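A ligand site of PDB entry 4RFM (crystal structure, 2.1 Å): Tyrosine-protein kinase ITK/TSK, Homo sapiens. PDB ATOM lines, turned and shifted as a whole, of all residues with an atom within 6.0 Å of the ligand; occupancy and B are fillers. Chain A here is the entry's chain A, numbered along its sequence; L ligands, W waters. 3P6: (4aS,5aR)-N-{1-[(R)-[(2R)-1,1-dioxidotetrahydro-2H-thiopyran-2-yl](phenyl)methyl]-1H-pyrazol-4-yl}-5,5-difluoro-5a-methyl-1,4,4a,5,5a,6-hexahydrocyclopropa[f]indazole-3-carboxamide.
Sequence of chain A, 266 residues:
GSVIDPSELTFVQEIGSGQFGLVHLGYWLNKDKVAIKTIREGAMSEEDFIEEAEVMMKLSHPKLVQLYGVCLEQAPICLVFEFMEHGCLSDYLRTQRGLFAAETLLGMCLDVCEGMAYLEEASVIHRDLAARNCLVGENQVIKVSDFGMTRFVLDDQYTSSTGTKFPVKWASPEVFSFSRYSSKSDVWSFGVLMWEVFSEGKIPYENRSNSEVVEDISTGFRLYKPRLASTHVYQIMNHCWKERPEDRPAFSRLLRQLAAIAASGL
Water W2 bridges N13 of the ligand and N of Gly 16. Water W1 bridges an oxygen (O23) of the ligand (2.9 Å) and a ring nitrogen (ND1) of His 86 (3.0 Å).
NE2 of Gln 13 touches C29 of the ligand, 3.9 Å away. Ile 15 touches the ligand (CG2 to C29, 3.6 Å). Gly 16 touches the ligand (N to C12, 3.9 Å). Phe 20 touches the ligand (CG to C33, 3.6 Å). Val 23 touches the ligand. CD2 of Leu 25 touches C28 of the ligand, 3.96 Å away. CB of Ala 35 touches N5 of the ligand (3.4 Å). Lys 37 touches the ligand (CB to F36, 3.5 Å). Phe 81 touches the ligand. CZ of Phe 83 touches C26 of the ligand (3.7 Å). Glu 85 touches the ligand. His 86 touches the ligand. Gly 87 touches the ligand. Leu 135 touches the ligand. OG of Ser 145 touches C1 of the ligand (3.3 Å). Hydrophobic or aromatic side chains that line the ligand: Ile 15, Phe 20, Val 23, Leu 25, Ala 35, Phe 81, Phe 83, Met 84 and Leu 135. Of the 24 residues printed, 17 come within 4 Å of the ligand. Along chain A the residues within 4 Å of the ligand span positions 13 to 145.
N of Leu 25 is in hydrogen-bond range of O of Gln 13 (2.8 Å). N of Phe 81 is in hydrogen-bond range of O of Ala 35, at 2.8 Å. O of Val 23 lies within hydrogen-bond range of N of Ile 15 (3.0 Å). The backbone NH (N) of Lys 37 sits at hydrogen-bond distance from the backbone carbonyl oxygen (O) of Leu 79 (2.8 Å). The side-chain amino group (NZ) of Lys 37 lies within hydrogen-bond range of the backbone carbonyl oxygen (O) of Phe 20 (3.3 Å).
A nitrogen (N5) of the ligand lies within hydrogen-bond range of the backbone carbonyl oxygen (O) of Glu 82 (2.7 Å). A nitrogen (N6) of the ligand is in hydrogen-bond range of the backbone NH (N) of Met 84, 3.0 Å away. O of Met 84 is in hydrogen-bond range of N10 of the ligand (3.0 Å).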
ATOM      1  N   GLN A  13       1.203  -7.129  -4.137  1.00  0.00           N
ATOM      2  CA  GLN A  13       1.424  -5.749  -4.378  1.00  0.00           C
ATOM      3  C   GLN A  13       1.393  -4.962  -3.058  1.00  0.00           C
ATOM      4  O   GLN A  13       0.753  -5.346  -2.101  1.00  0.00           O
ATOM      5  CB  GLN A  13       0.301  -5.281  -5.320  1.00  0.00           C
ATOM      6  CG  GLN A  13      -0.926  -4.771  -4.592  1.00  0.00           C
ATOM      7  CD  GLN A  13      -2.235  -5.172  -5.221  1.00  0.00           C
ATOM      8  OE1 GLN A  13      -2.501  -6.351  -5.432  1.00  0.00           O
ATOM      9  NE2 GLN A  13      -3.079  -4.194  -5.456  1.00  0.00           N
ATOM     10  N   ILE A  15       0.044  -2.199  -0.603  1.00  0.00           N
ATOM     11  CA  ILE A  15      -1.278  -1.643  -0.354  1.00  0.00           C
ATOM     12  C   ILE A  15      -1.116  -0.651   0.782  1.00  0.00           C
ATOM     13  O   ILE A  15      -0.137  -0.703   1.514  1.00  0.00           O
ATOM     14  CB  ILE A  15      -2.364  -2.734  -0.023  1.00  0.00           C
ATOM     15  CG1 ILE A  15      -2.052  -3.446   1.303  1.00  0.00           C
ATOM     16  CG2 ILE A  15      -2.563  -3.684  -1.227  1.00  0.00           C
ATOM     17  CD1 ILE A  15      -2.916  -4.636   1.592  1.00  0.00           C
ATOM     18  N   GLY A  16      -2.083   0.269   0.896  1.00  0.00           N
ATOM     19  CA  GLY A  16      -2.101   1.219   2.013  1.00  0.00           C
ATOM     20  C   GLY A  16      -1.366   2.523   1.731  1.00  0.00           C
ATOM     21  O   GLY A  16      -0.579   2.647   0.785  1.00  0.00           O
ATOM     22  N   PHE A  20       0.571   2.156   8.393  1.00  0.00           N
ATOM     23  CA  PHE A  20       1.136   0.955   9.024  1.00  0.00           C
ATOM     24  C   PHE A  20       2.505   0.507   8.398  1.00  0.00           C
ATOM     25  O   PHE A  20       2.931  -0.628   8.590  1.00  0.00           O
ATOM     26  CB  PHE A  20       0.130  -0.196   8.969  1.00  0.00           C
ATOM     27  CG  PHE A  20      -1.181   0.129   9.613  1.00  0.00           C
ATOM     28  CD1 PHE A  20      -1.387  -0.095  10.974  1.00  0.00           C
ATOM     29  CD2 PHE A  20      -2.246   0.620   8.876  1.00  0.00           C
ATOM     30  CE1 PHE A  20      -2.609   0.177  11.574  1.00  0.00           C
ATOM     31  CE2 PHE A  20      -3.483   0.884   9.473  1.00  0.00           C
ATOM     32  CZ  PHE A  20      -3.661   0.661  10.820  1.00  0.00           C
ATOM     33  N   VAL A  23       3.291  -2.625   3.741  1.00  0.00           N
ATOM     34  CA  VAL A  23       2.315  -3.692   3.747  1.00  0.00           C
ATOM     35  C   VAL A  23       2.151  -4.172   2.318  1.00  0.00           C
ATOM     36  O   VAL A  23       2.041  -3.326   1.399  1.00  0.00           O
ATOM     37  CB  VAL A  23       0.926  -3.197   4.262  1.00  0.00           C
ATOM     38  CG1 VAL A  23      -0.085  -4.320   4.418  1.00  0.00           C
ATOM     39  CG2 VAL A  23       1.064  -2.561   5.619  1.00  0.00           C
ATOM     40  N   HIS A  24       2.137  -5.498   2.148  1.00  0.00           N
ATOM     41  CA  HIS A  24       1.701  -6.123   0.909  1.00  0.00           C
ATOM     42  C   HIS A  24       0.380  -6.857   1.052  1.00  0.00           C
ATOM     43  O   HIS A  24       0.060  -7.346   2.099  1.00  0.00           O
ATOM     44  CB  HIS A  24       2.742  -7.134   0.449  1.00  0.00           C
ATOM     45  CG  HIS A  24       4.026  -6.495   0.049  1.00  0.00           C
ATOM     46  ND1 HIS A  24       4.402  -6.350  -1.277  1.00  0.00           N
ATOM     47  CD2 HIS A  24       5.002  -5.931   0.785  1.00  0.00           C
ATOM     48  CE1 HIS A  24       5.572  -5.748  -1.325  1.00  0.00           C
ATOM     49  NE2 HIS A  24       5.962  -5.498  -0.097  1.00  0.00           N
ATOM     50  N   LEU A  25      -0.378  -6.911  -0.048  1.00  0.00           N
ATOM     51  CA  LEU A  25      -1.420  -7.920  -0.189  1.00  0.00           C
ATOM     52  C   LEU A  25      -0.723  -9.278  -0.366  1.00  0.00           C
ATOM     53  O   LEU A  25       0.238  -9.384  -1.096  1.00  0.00           O
ATOM     54  CB  LEU A  25      -2.332  -7.611  -1.393  1.00  0.00           C
ATOM     55  CG  LEU A  25      -3.445  -8.580  -1.711  1.00  0.00           C
ATOM     56  CD1 LEU A  25      -4.345  -8.724  -0.505  1.00  0.00           C
ATOM     57  CD2 LEU A  25      -4.271  -8.103  -2.895  1.00  0.00           C
ATOM     58  N   LYS A  33      -6.522 -14.487   1.242  1.00  0.00           N
ATOM     59  CA  LYS A  33      -5.905 -13.137   1.267  1.00  0.00           C
ATOM     60  C   LYS A  33      -5.456 -12.722   2.672  1.00  0.00           C
ATOM     61  O   LYS A  33      -6.198 -12.877   3.614  1.00  0.00           O
ATOM     62  CB  LYS A  33      -6.831 -12.098   0.735  1.00  0.00           C
ATOM     63  CG  LYS A  33      -6.752 -11.916  -0.760  1.00  0.00           C
ATOM     64  CD  LYS A  33      -8.098 -11.579  -1.348  1.00  0.00           C
ATOM     65  CE  LYS A  33      -8.738 -10.416  -0.613  1.00  0.00           C
ATOM     66  NZ  LYS A  33      -9.931  -9.930  -1.356  1.00  0.00           N
ATOM     67  N   ALA A  35      -2.771  -9.572   4.766  1.00  0.00           N
ATOM     68  CA  ALA A  35      -1.971  -8.387   4.678  1.00  0.00           C
ATOM     69  C   ALA A  35      -0.643  -8.765   5.337  1.00  0.00           C
ATOM     70  O   ALA A  35      -0.608  -9.329   6.454  1.00  0.00           O
ATOM     71  CB  ALA A  35      -2.630  -7.268   5.429  1.00  0.00           C
ATOM     72  N   ILE A  36       0.432  -8.532   4.615  1.00  0.00           N
ATOM     73  CA  ILE A  36       1.751  -8.833   5.164  1.00  0.00           C
ATOM     74  C   ILE A  36       2.495  -7.564   5.446  1.00  0.00           C
ATOM     75  O   ILE A  36       2.654  -6.694   4.585  1.00  0.00           O
ATOM     76  CB  ILE A  36       2.581  -9.736   4.248  1.00  0.00           C
ATOM     77  CG1 ILE A  36       1.830 -11.055   3.933  1.00  0.00           C
ATOM     78  CG2 ILE A  36       3.972  -9.987   4.877  1.00  0.00           C
ATOM     79  CD1 ILE A  36       2.464 -11.930   2.824  1.00  0.00           C
ATOM     80  N   LYS A  37       3.014  -7.483   6.654  1.00  0.00           N
ATOM     81  CA  LYS A  37       3.671  -6.296   7.037  1.00  0.00           C
ATOM     82  C   LYS A  37       5.153  -6.584   7.371  1.00  0.00           C
ATOM     83  O   LYS A  37       5.480  -7.373   8.278  1.00  0.00           O
ATOM     84  CB  LYS A  37       2.904  -5.678   8.188  1.00  0.00           C
ATOM     85  CG  LYS A  37       3.542  -4.387   8.662  1.00  0.00           C
ATOM     86  CD  LYS A  37       4.415  -4.659   9.855  1.00  0.00           C
ATOM     87  CE  LYS A  37       3.780  -4.039  11.077  1.00  0.00           C
ATOM     88  NZ  LYS A  37       4.038  -2.569  10.960  1.00  0.00           N
ATOM     89  N   VAL A  65      -8.478  -6.719  14.484  1.00  0.00           N
ATOM     90  CA  VAL A  65      -7.757  -7.264  13.330  1.00  0.00           C
ATOM     91  C   VAL A  65      -6.798  -8.352  13.788  1.00  0.00           C
ATOM     92  O   VAL A  65      -5.906  -8.092  14.585  1.00  0.00           O
ATOM     93  CB  VAL A  65      -6.931  -6.196  12.611  1.00  0.00           C
ATOM     94  CG1 VAL A  65      -6.296  -6.817  11.388  1.00  0.00           C
ATOM     95  CG2 VAL A  65      -7.792  -4.998  12.165  1.00  0.00           C
ATOM     96  N   LEU A  79       4.966  -9.767   9.715  1.00  0.00           N
ATOM     97  CA  LEU A  79       3.691 -10.096  10.358  1.00  0.00           C
ATOM     98  C   LEU A  79       2.612 -10.413   9.291  1.00  0.00           C
ATOM     99  O   LEU A  79       2.448  -9.656   8.313  1.00  0.00           O
ATOM    100  CB  LEU A  79       3.255  -8.913  11.240  1.00  0.00           C
ATOM    101  CG  LEU A  79       4.356  -8.379  12.190  1.00  0.00           C
ATOM    102  CD1 LEU A  79       3.897  -7.198  13.048  1.00  0.00           C
ATOM    103  CD2 LEU A  79       4.811  -9.547  13.048  1.00  0.00           C
ATOM    104  N   PHE A  81      -1.315 -10.751   8.762  1.00  0.00           N
ATOM    105  CA  PHE A  81      -2.528 -10.232   9.381  1.00  0.00           C
ATOM    106  C   PHE A  81      -3.729 -10.579   8.533  1.00  0.00           C
ATOM    107  O   PHE A  81      -3.627 -10.873   7.326  1.00  0.00           O
ATOM    108  CB  PHE A  81      -2.487  -8.701   9.512  1.00  0.00           C
ATOM    109  CG  PHE A  81      -1.614  -8.185  10.608  1.00  0.00           C
ATOM    110  CD1 PHE A  81      -0.380  -7.618  10.334  1.00  0.00           C
ATOM    111  CD2 PHE A  81      -2.035  -8.258  11.932  1.00  0.00           C
ATOM    112  CE1 PHE A  81       0.423  -7.142  11.347  1.00  0.00           C
ATOM    113  CE2 PHE A  81      -1.241  -7.780  12.949  1.00  0.00           C
ATOM    114  CZ  PHE A  81      -0.016  -7.192  12.665  1.00  0.00           C
ATOM    115  N   GLU A  82      -4.879 -10.530   9.183  1.00  0.00           N
ATOM    116  CA  GLU A  82      -6.154 -10.448   8.530  1.00  0.00           C
ATOM    117  C   GLU A  82      -6.180  -9.331   7.466  1.00  0.00           C
ATOM    118  O   GLU A  82      -5.888  -8.160   7.745  1.00  0.00           O
ATOM    119  CB  GLU A  82      -7.228 -10.193   9.634  1.00  0.00           C
ATOM    120  CG  GLU A  82      -8.670 -10.130   9.165  1.00  0.00           C
ATOM    121  CD  GLU A  82      -9.677  -9.945  10.294  1.00  0.00           C
ATOM    122  OE1 GLU A  82     -10.879  -9.813   9.911  1.00  0.00           O
ATOM    123  OE2 GLU A  82      -9.321  -9.894  11.541  1.00  0.00           O
ATOM    124  N   PHE A  83      -6.589  -9.682   6.243  1.00  0.00           N
ATOM    125  CA  PHE A  83      -6.783  -8.663   5.232  1.00  0.00           C
ATOM    126  C   PHE A  83      -8.088  -7.915   5.427  1.00  0.00           C
ATOM    127  O   PHE A  83      -9.121  -8.529   5.568  1.00  0.00           O
ATOM    128  CB  PHE A  83      -6.702  -9.261   3.831  1.00  0.00           C
ATOM    129  CG  PHE A  83      -6.934  -8.257   2.740  1.00  0.00           C
ATOM    130  CD1 PHE A  83      -6.010  -7.283   2.518  1.00  0.00           C
ATOM    131  CD2 PHE A  83      -8.132  -8.255   2.008  1.00  0.00           C
ATOM    132  CE1 PHE A  83      -6.224  -6.341   1.519  1.00  0.00           C
ATOM    133  CE2 PHE A  83      -8.337  -7.334   1.020  1.00  0.00           C
ATOM    134  CZ  PHE A  83      -7.395  -6.371   0.769  1.00  0.00           C
ATOM    135  N   MET A  84      -8.032  -6.575   5.417  1.00  0.00           N
ATOM    136  CA  MET A  84      -9.172  -5.719   5.625  1.00  0.00           C
ATOM    137  C   MET A  84      -9.537  -4.967   4.329  1.00  0.00           C
ATOM    138  O   MET A  84      -8.861  -4.055   3.888  1.00  0.00           O
ATOM    139  CB  MET A  84      -8.886  -4.722   6.757  1.00  0.00           C
ATOM    140  CG  MET A  84      -8.583  -5.407   8.094  1.00  0.00           C
ATOM    141  SD  MET A  84      -9.979  -6.271   8.779  1.00  0.00           S
ATOM    142  CE  MET A  84     -11.028  -4.908   9.246  1.00  0.00           C
ATOM    143  N   GLU A  85     -10.648  -5.354   3.783  1.00  0.00           N
ATOM    144  CA  GLU A  85     -11.052  -5.048   2.416  1.00  0.00           C
ATOM    145  C   GLU A  85     -10.998  -3.569   2.102  1.00  0.00           C
ATOM    146  O   GLU A  85     -10.614  -3.171   1.006  1.00  0.00           O
ATOM    147  CB  GLU A  85     -12.465  -5.614   2.259  1.00  0.00           C
ATOM    148  CG  GLU A  85     -13.041  -5.776   0.868  1.00  0.00           C
ATOM    149  CD  GLU A  85     -14.210  -6.758   0.917  1.00  0.00           C
ATOM    150  OE1 GLU A  85     -14.536  -7.207   2.027  1.00  0.00           O
ATOM    151  OE2 GLU A  85     -14.794  -7.100  -0.136  1.00  0.00           O
ATOM    152  N   HIS A  86     -11.346  -2.727   3.081  1.00  0.00           N
ATOM    153  CA  HIS A  86     -11.558  -1.310   2.803  1.00  0.00           C
ATOM    154  C   HIS A  86     -10.600  -0.372   3.503  1.00  0.00           C
ATOM    155  O   HIS A  86     -10.912   0.803   3.687  1.00  0.00           O
ATOM    156  CB  HIS A  86     -12.986  -0.919   3.143  1.00  0.00           C
ATOM    157  CG  HIS A  86     -14.032  -1.710   2.414  1.00  0.00           C
ATOM    158  ND1 HIS A  86     -14.218  -1.607   1.048  1.00  0.00           N
ATOM    159  CD2 HIS A  86     -14.954  -2.589   2.865  1.00  0.00           C
ATOM    160  CE1 HIS A  86     -15.227  -2.393   0.704  1.00  0.00           C
ATOM    161  NE2 HIS A  86     -15.684  -2.994   1.782  1.00  0.00           N
ATOM    162  N   GLY A  87      -9.420  -0.873   3.873  1.00  0.00           N
ATOM    163  CA  GLY A  87      -8.327   0.001   4.217  1.00  0.00           C
ATOM    164  C   GLY A  87      -8.471   0.682   5.565  1.00  0.00           C
ATOM    165  O   GLY A  87      -9.212   0.185   6.422  1.00  0.00           O
ATOM    166  N   CYS A  88      -7.755   1.784   5.722  1.00  0.00           N
ATOM    167  CA  CYS A  88      -7.649   2.547   6.981  1.00  0.00           C
ATOM    168  C   CYS A  88      -8.860   3.465   7.134  1.00  0.00           C
ATOM    169  O   CYS A  88      -9.264   4.125   6.198  1.00  0.00           O
ATOM    170  CB  CYS A  88      -6.343   3.323   7.017  1.00  0.00           C
ATOM    171  SG  CYS A  88      -6.085   4.298   8.503  1.00  0.00           S
ATOM    172  N   LEU A 135      -9.195  -0.241  11.023  1.00  0.00           N
ATOM    173  CA  LEU A 135      -9.322  -0.705   9.641  1.00  0.00           C
ATOM    174  C   LEU A 135     -10.756  -1.127   9.378  1.00  0.00           C
ATOM    175  O   LEU A 135     -11.512  -1.434  10.298  1.00  0.00           O
ATOM    176  CB  LEU A 135      -8.372  -1.848   9.362  1.00  0.00           C
ATOM    177  CG  LEU A 135      -6.922  -1.455   9.117  1.00  0.00           C
ATOM    178  CD1 LEU A 135      -5.984  -2.591   9.537  1.00  0.00           C
ATOM    179  CD2 LEU A 135      -6.627  -1.051   7.670  1.00  0.00           C
ATOM    180  N   SER A 145      -6.740  -2.144  15.481  1.00  0.00           N
ATOM    181  CA  SER A 145      -5.436  -2.749  15.307  1.00  0.00           C
ATOM    182  C   SER A 145      -4.411  -2.057  16.198  1.00  0.00           C
ATOM    183  O   SER A 145      -4.762  -1.212  17.032  1.00  0.00           O
ATOM    184  CB  SER A 145      -5.035  -2.634  13.850  1.00  0.00           C
ATOM    185  OG  SER A 145      -4.001  -3.586  13.597  1.00  0.00           O
ATOM    186  N   ASP A 146      -3.133  -2.433  16.028  1.00  0.00           N
ATOM    187  CA  ASP A 146      -2.012  -1.845  16.769  1.00  0.00           C
ATOM    188  C   ASP A 146      -2.069  -2.030  18.266  1.00  0.00           C
ATOM    189  O   ASP A 146      -1.605  -1.177  19.013  1.00  0.00           O
ATOM    190  CB  ASP A 146      -1.878  -0.330  16.455  1.00  0.00           C
ATOM    191  CG  ASP A 146      -0.494   0.225  16.741  1.00  0.00           C
ATOM    192  OD1 ASP A 146       0.484  -0.526  16.523  1.00  0.00           O
ATOM    193  OD2 ASP A 146      -0.401   1.429  17.142  1.00  0.00           O
HETATM  194  C1  3P6 L   1      -2.469  -4.111  10.764  1.00  0.00           C
HETATM  195  C2  3P6 L   1      -2.477  -4.362   9.287  1.00  0.00           C
HETATM  196  C3  3P6 L   1      -3.486  -5.397   8.809  1.00  0.00           C
HETATM  197  C4  3P6 L   1      -4.157  -4.997   7.542  1.00  0.00           C
HETATM  198  N5  3P6 L   1      -5.176  -5.644   6.931  1.00  0.00           N
HETATM  199  N6  3P6 L   1      -5.544  -5.020   5.782  1.00  0.00           N
HETATM  200  C7  3P6 L   1      -4.745  -3.952   5.648  1.00  0.00           C
HETATM  201  C8  3P6 L   1      -4.844  -3.032   4.508  1.00  0.00           C
HETATM  202  O9  3P6 L   1      -4.008  -2.183   4.227  1.00  0.00           O
HETATM  203  N10 3P6 L   1      -5.988  -3.184   3.756  1.00  0.00           N
HETATM  204  C11 3P6 L   1      -6.188  -2.512   2.564  1.00  0.00           C
HETATM  205  C12 3P6 L   1      -5.469  -1.477   1.912  1.00  0.00           C
HETATM  206  N13 3P6 L   1      -5.983  -1.103   0.743  1.00  0.00           N
HETATM  207  N14 3P6 L   1      -7.068  -1.906   0.663  1.00  0.00           N
HETATM  208  C15 3P6 L   1      -7.226  -2.767   1.712  1.00  0.00           C
HETATM  209  C16 3P6 L   1      -7.946  -1.884  -0.483  1.00  0.00           C
HETATM  210  C17 3P6 L   1      -7.995  -0.541  -1.206  1.00  0.00           C
HETATM  211  C18 3P6 L   1      -8.851  -0.642  -2.475  1.00  0.00           C
HETATM  212  C19 3P6 L   1      -8.751   0.654  -3.294  1.00  0.00           C
HETATM  213  C20 3P6 L   1      -9.487   1.779  -2.653  1.00  0.00           C
HETATM  214  C21 3P6 L   1      -8.886   2.088  -1.289  1.00  0.00           C
HETATM  215  S22 3P6 L   1      -8.764   0.685  -0.152  1.00  0.00           S
HETATM  216  O23 3P6 L   1     -10.118   0.250   0.166  1.00  0.00           O
HETATM  217  O24 3P6 L   1      -7.823   1.074   0.879  1.00  0.00           O
HETATM  218  C25 3P6 L   1      -7.531  -2.984  -1.425  1.00  0.00           C
HETATM  219  C26 3P6 L   1      -8.438  -3.936  -1.831  1.00  0.00           C
HETATM  220  C27 3P6 L   1      -8.056  -4.947  -2.706  1.00  0.00           C
HETATM  221  C28 3P6 L   1      -6.753  -5.025  -3.155  1.00  0.00           C
HETATM  222  C29 3P6 L   1      -5.828  -4.079  -2.756  1.00  0.00           C
HETATM  223  C30 3P6 L   1      -6.221  -3.057  -1.889  1.00  0.00           C
HETATM  224  C31 3P6 L   1      -3.871  -3.909   6.761  1.00  0.00           C
HETATM  225  C32 3P6 L   1      -2.814  -2.947   7.084  1.00  0.00           C
HETATM  226  C33 3P6 L   1      -2.198  -3.142   8.441  1.00  0.00           C
HETATM  227  C34 3P6 L   1      -1.190  -4.238   8.563  1.00  0.00           C
HETATM  228  F35 3P6 L   1      -0.989  -5.193   7.563  1.00  0.00           F
HETATM  229  F36 3P6 L   1      -0.027  -4.064   9.291  1.00  0.00           F
HETATM  230  O   HOH W   1     -12.828   0.372  -0.732  1.00  0.00           O
HETATM  231  O   HOH W   2      -4.360   0.544  -0.763  1.00  0.00           O
HETATM  232  O   HOH W   3      -3.030   0.205   5.396  1.00  0.00           O
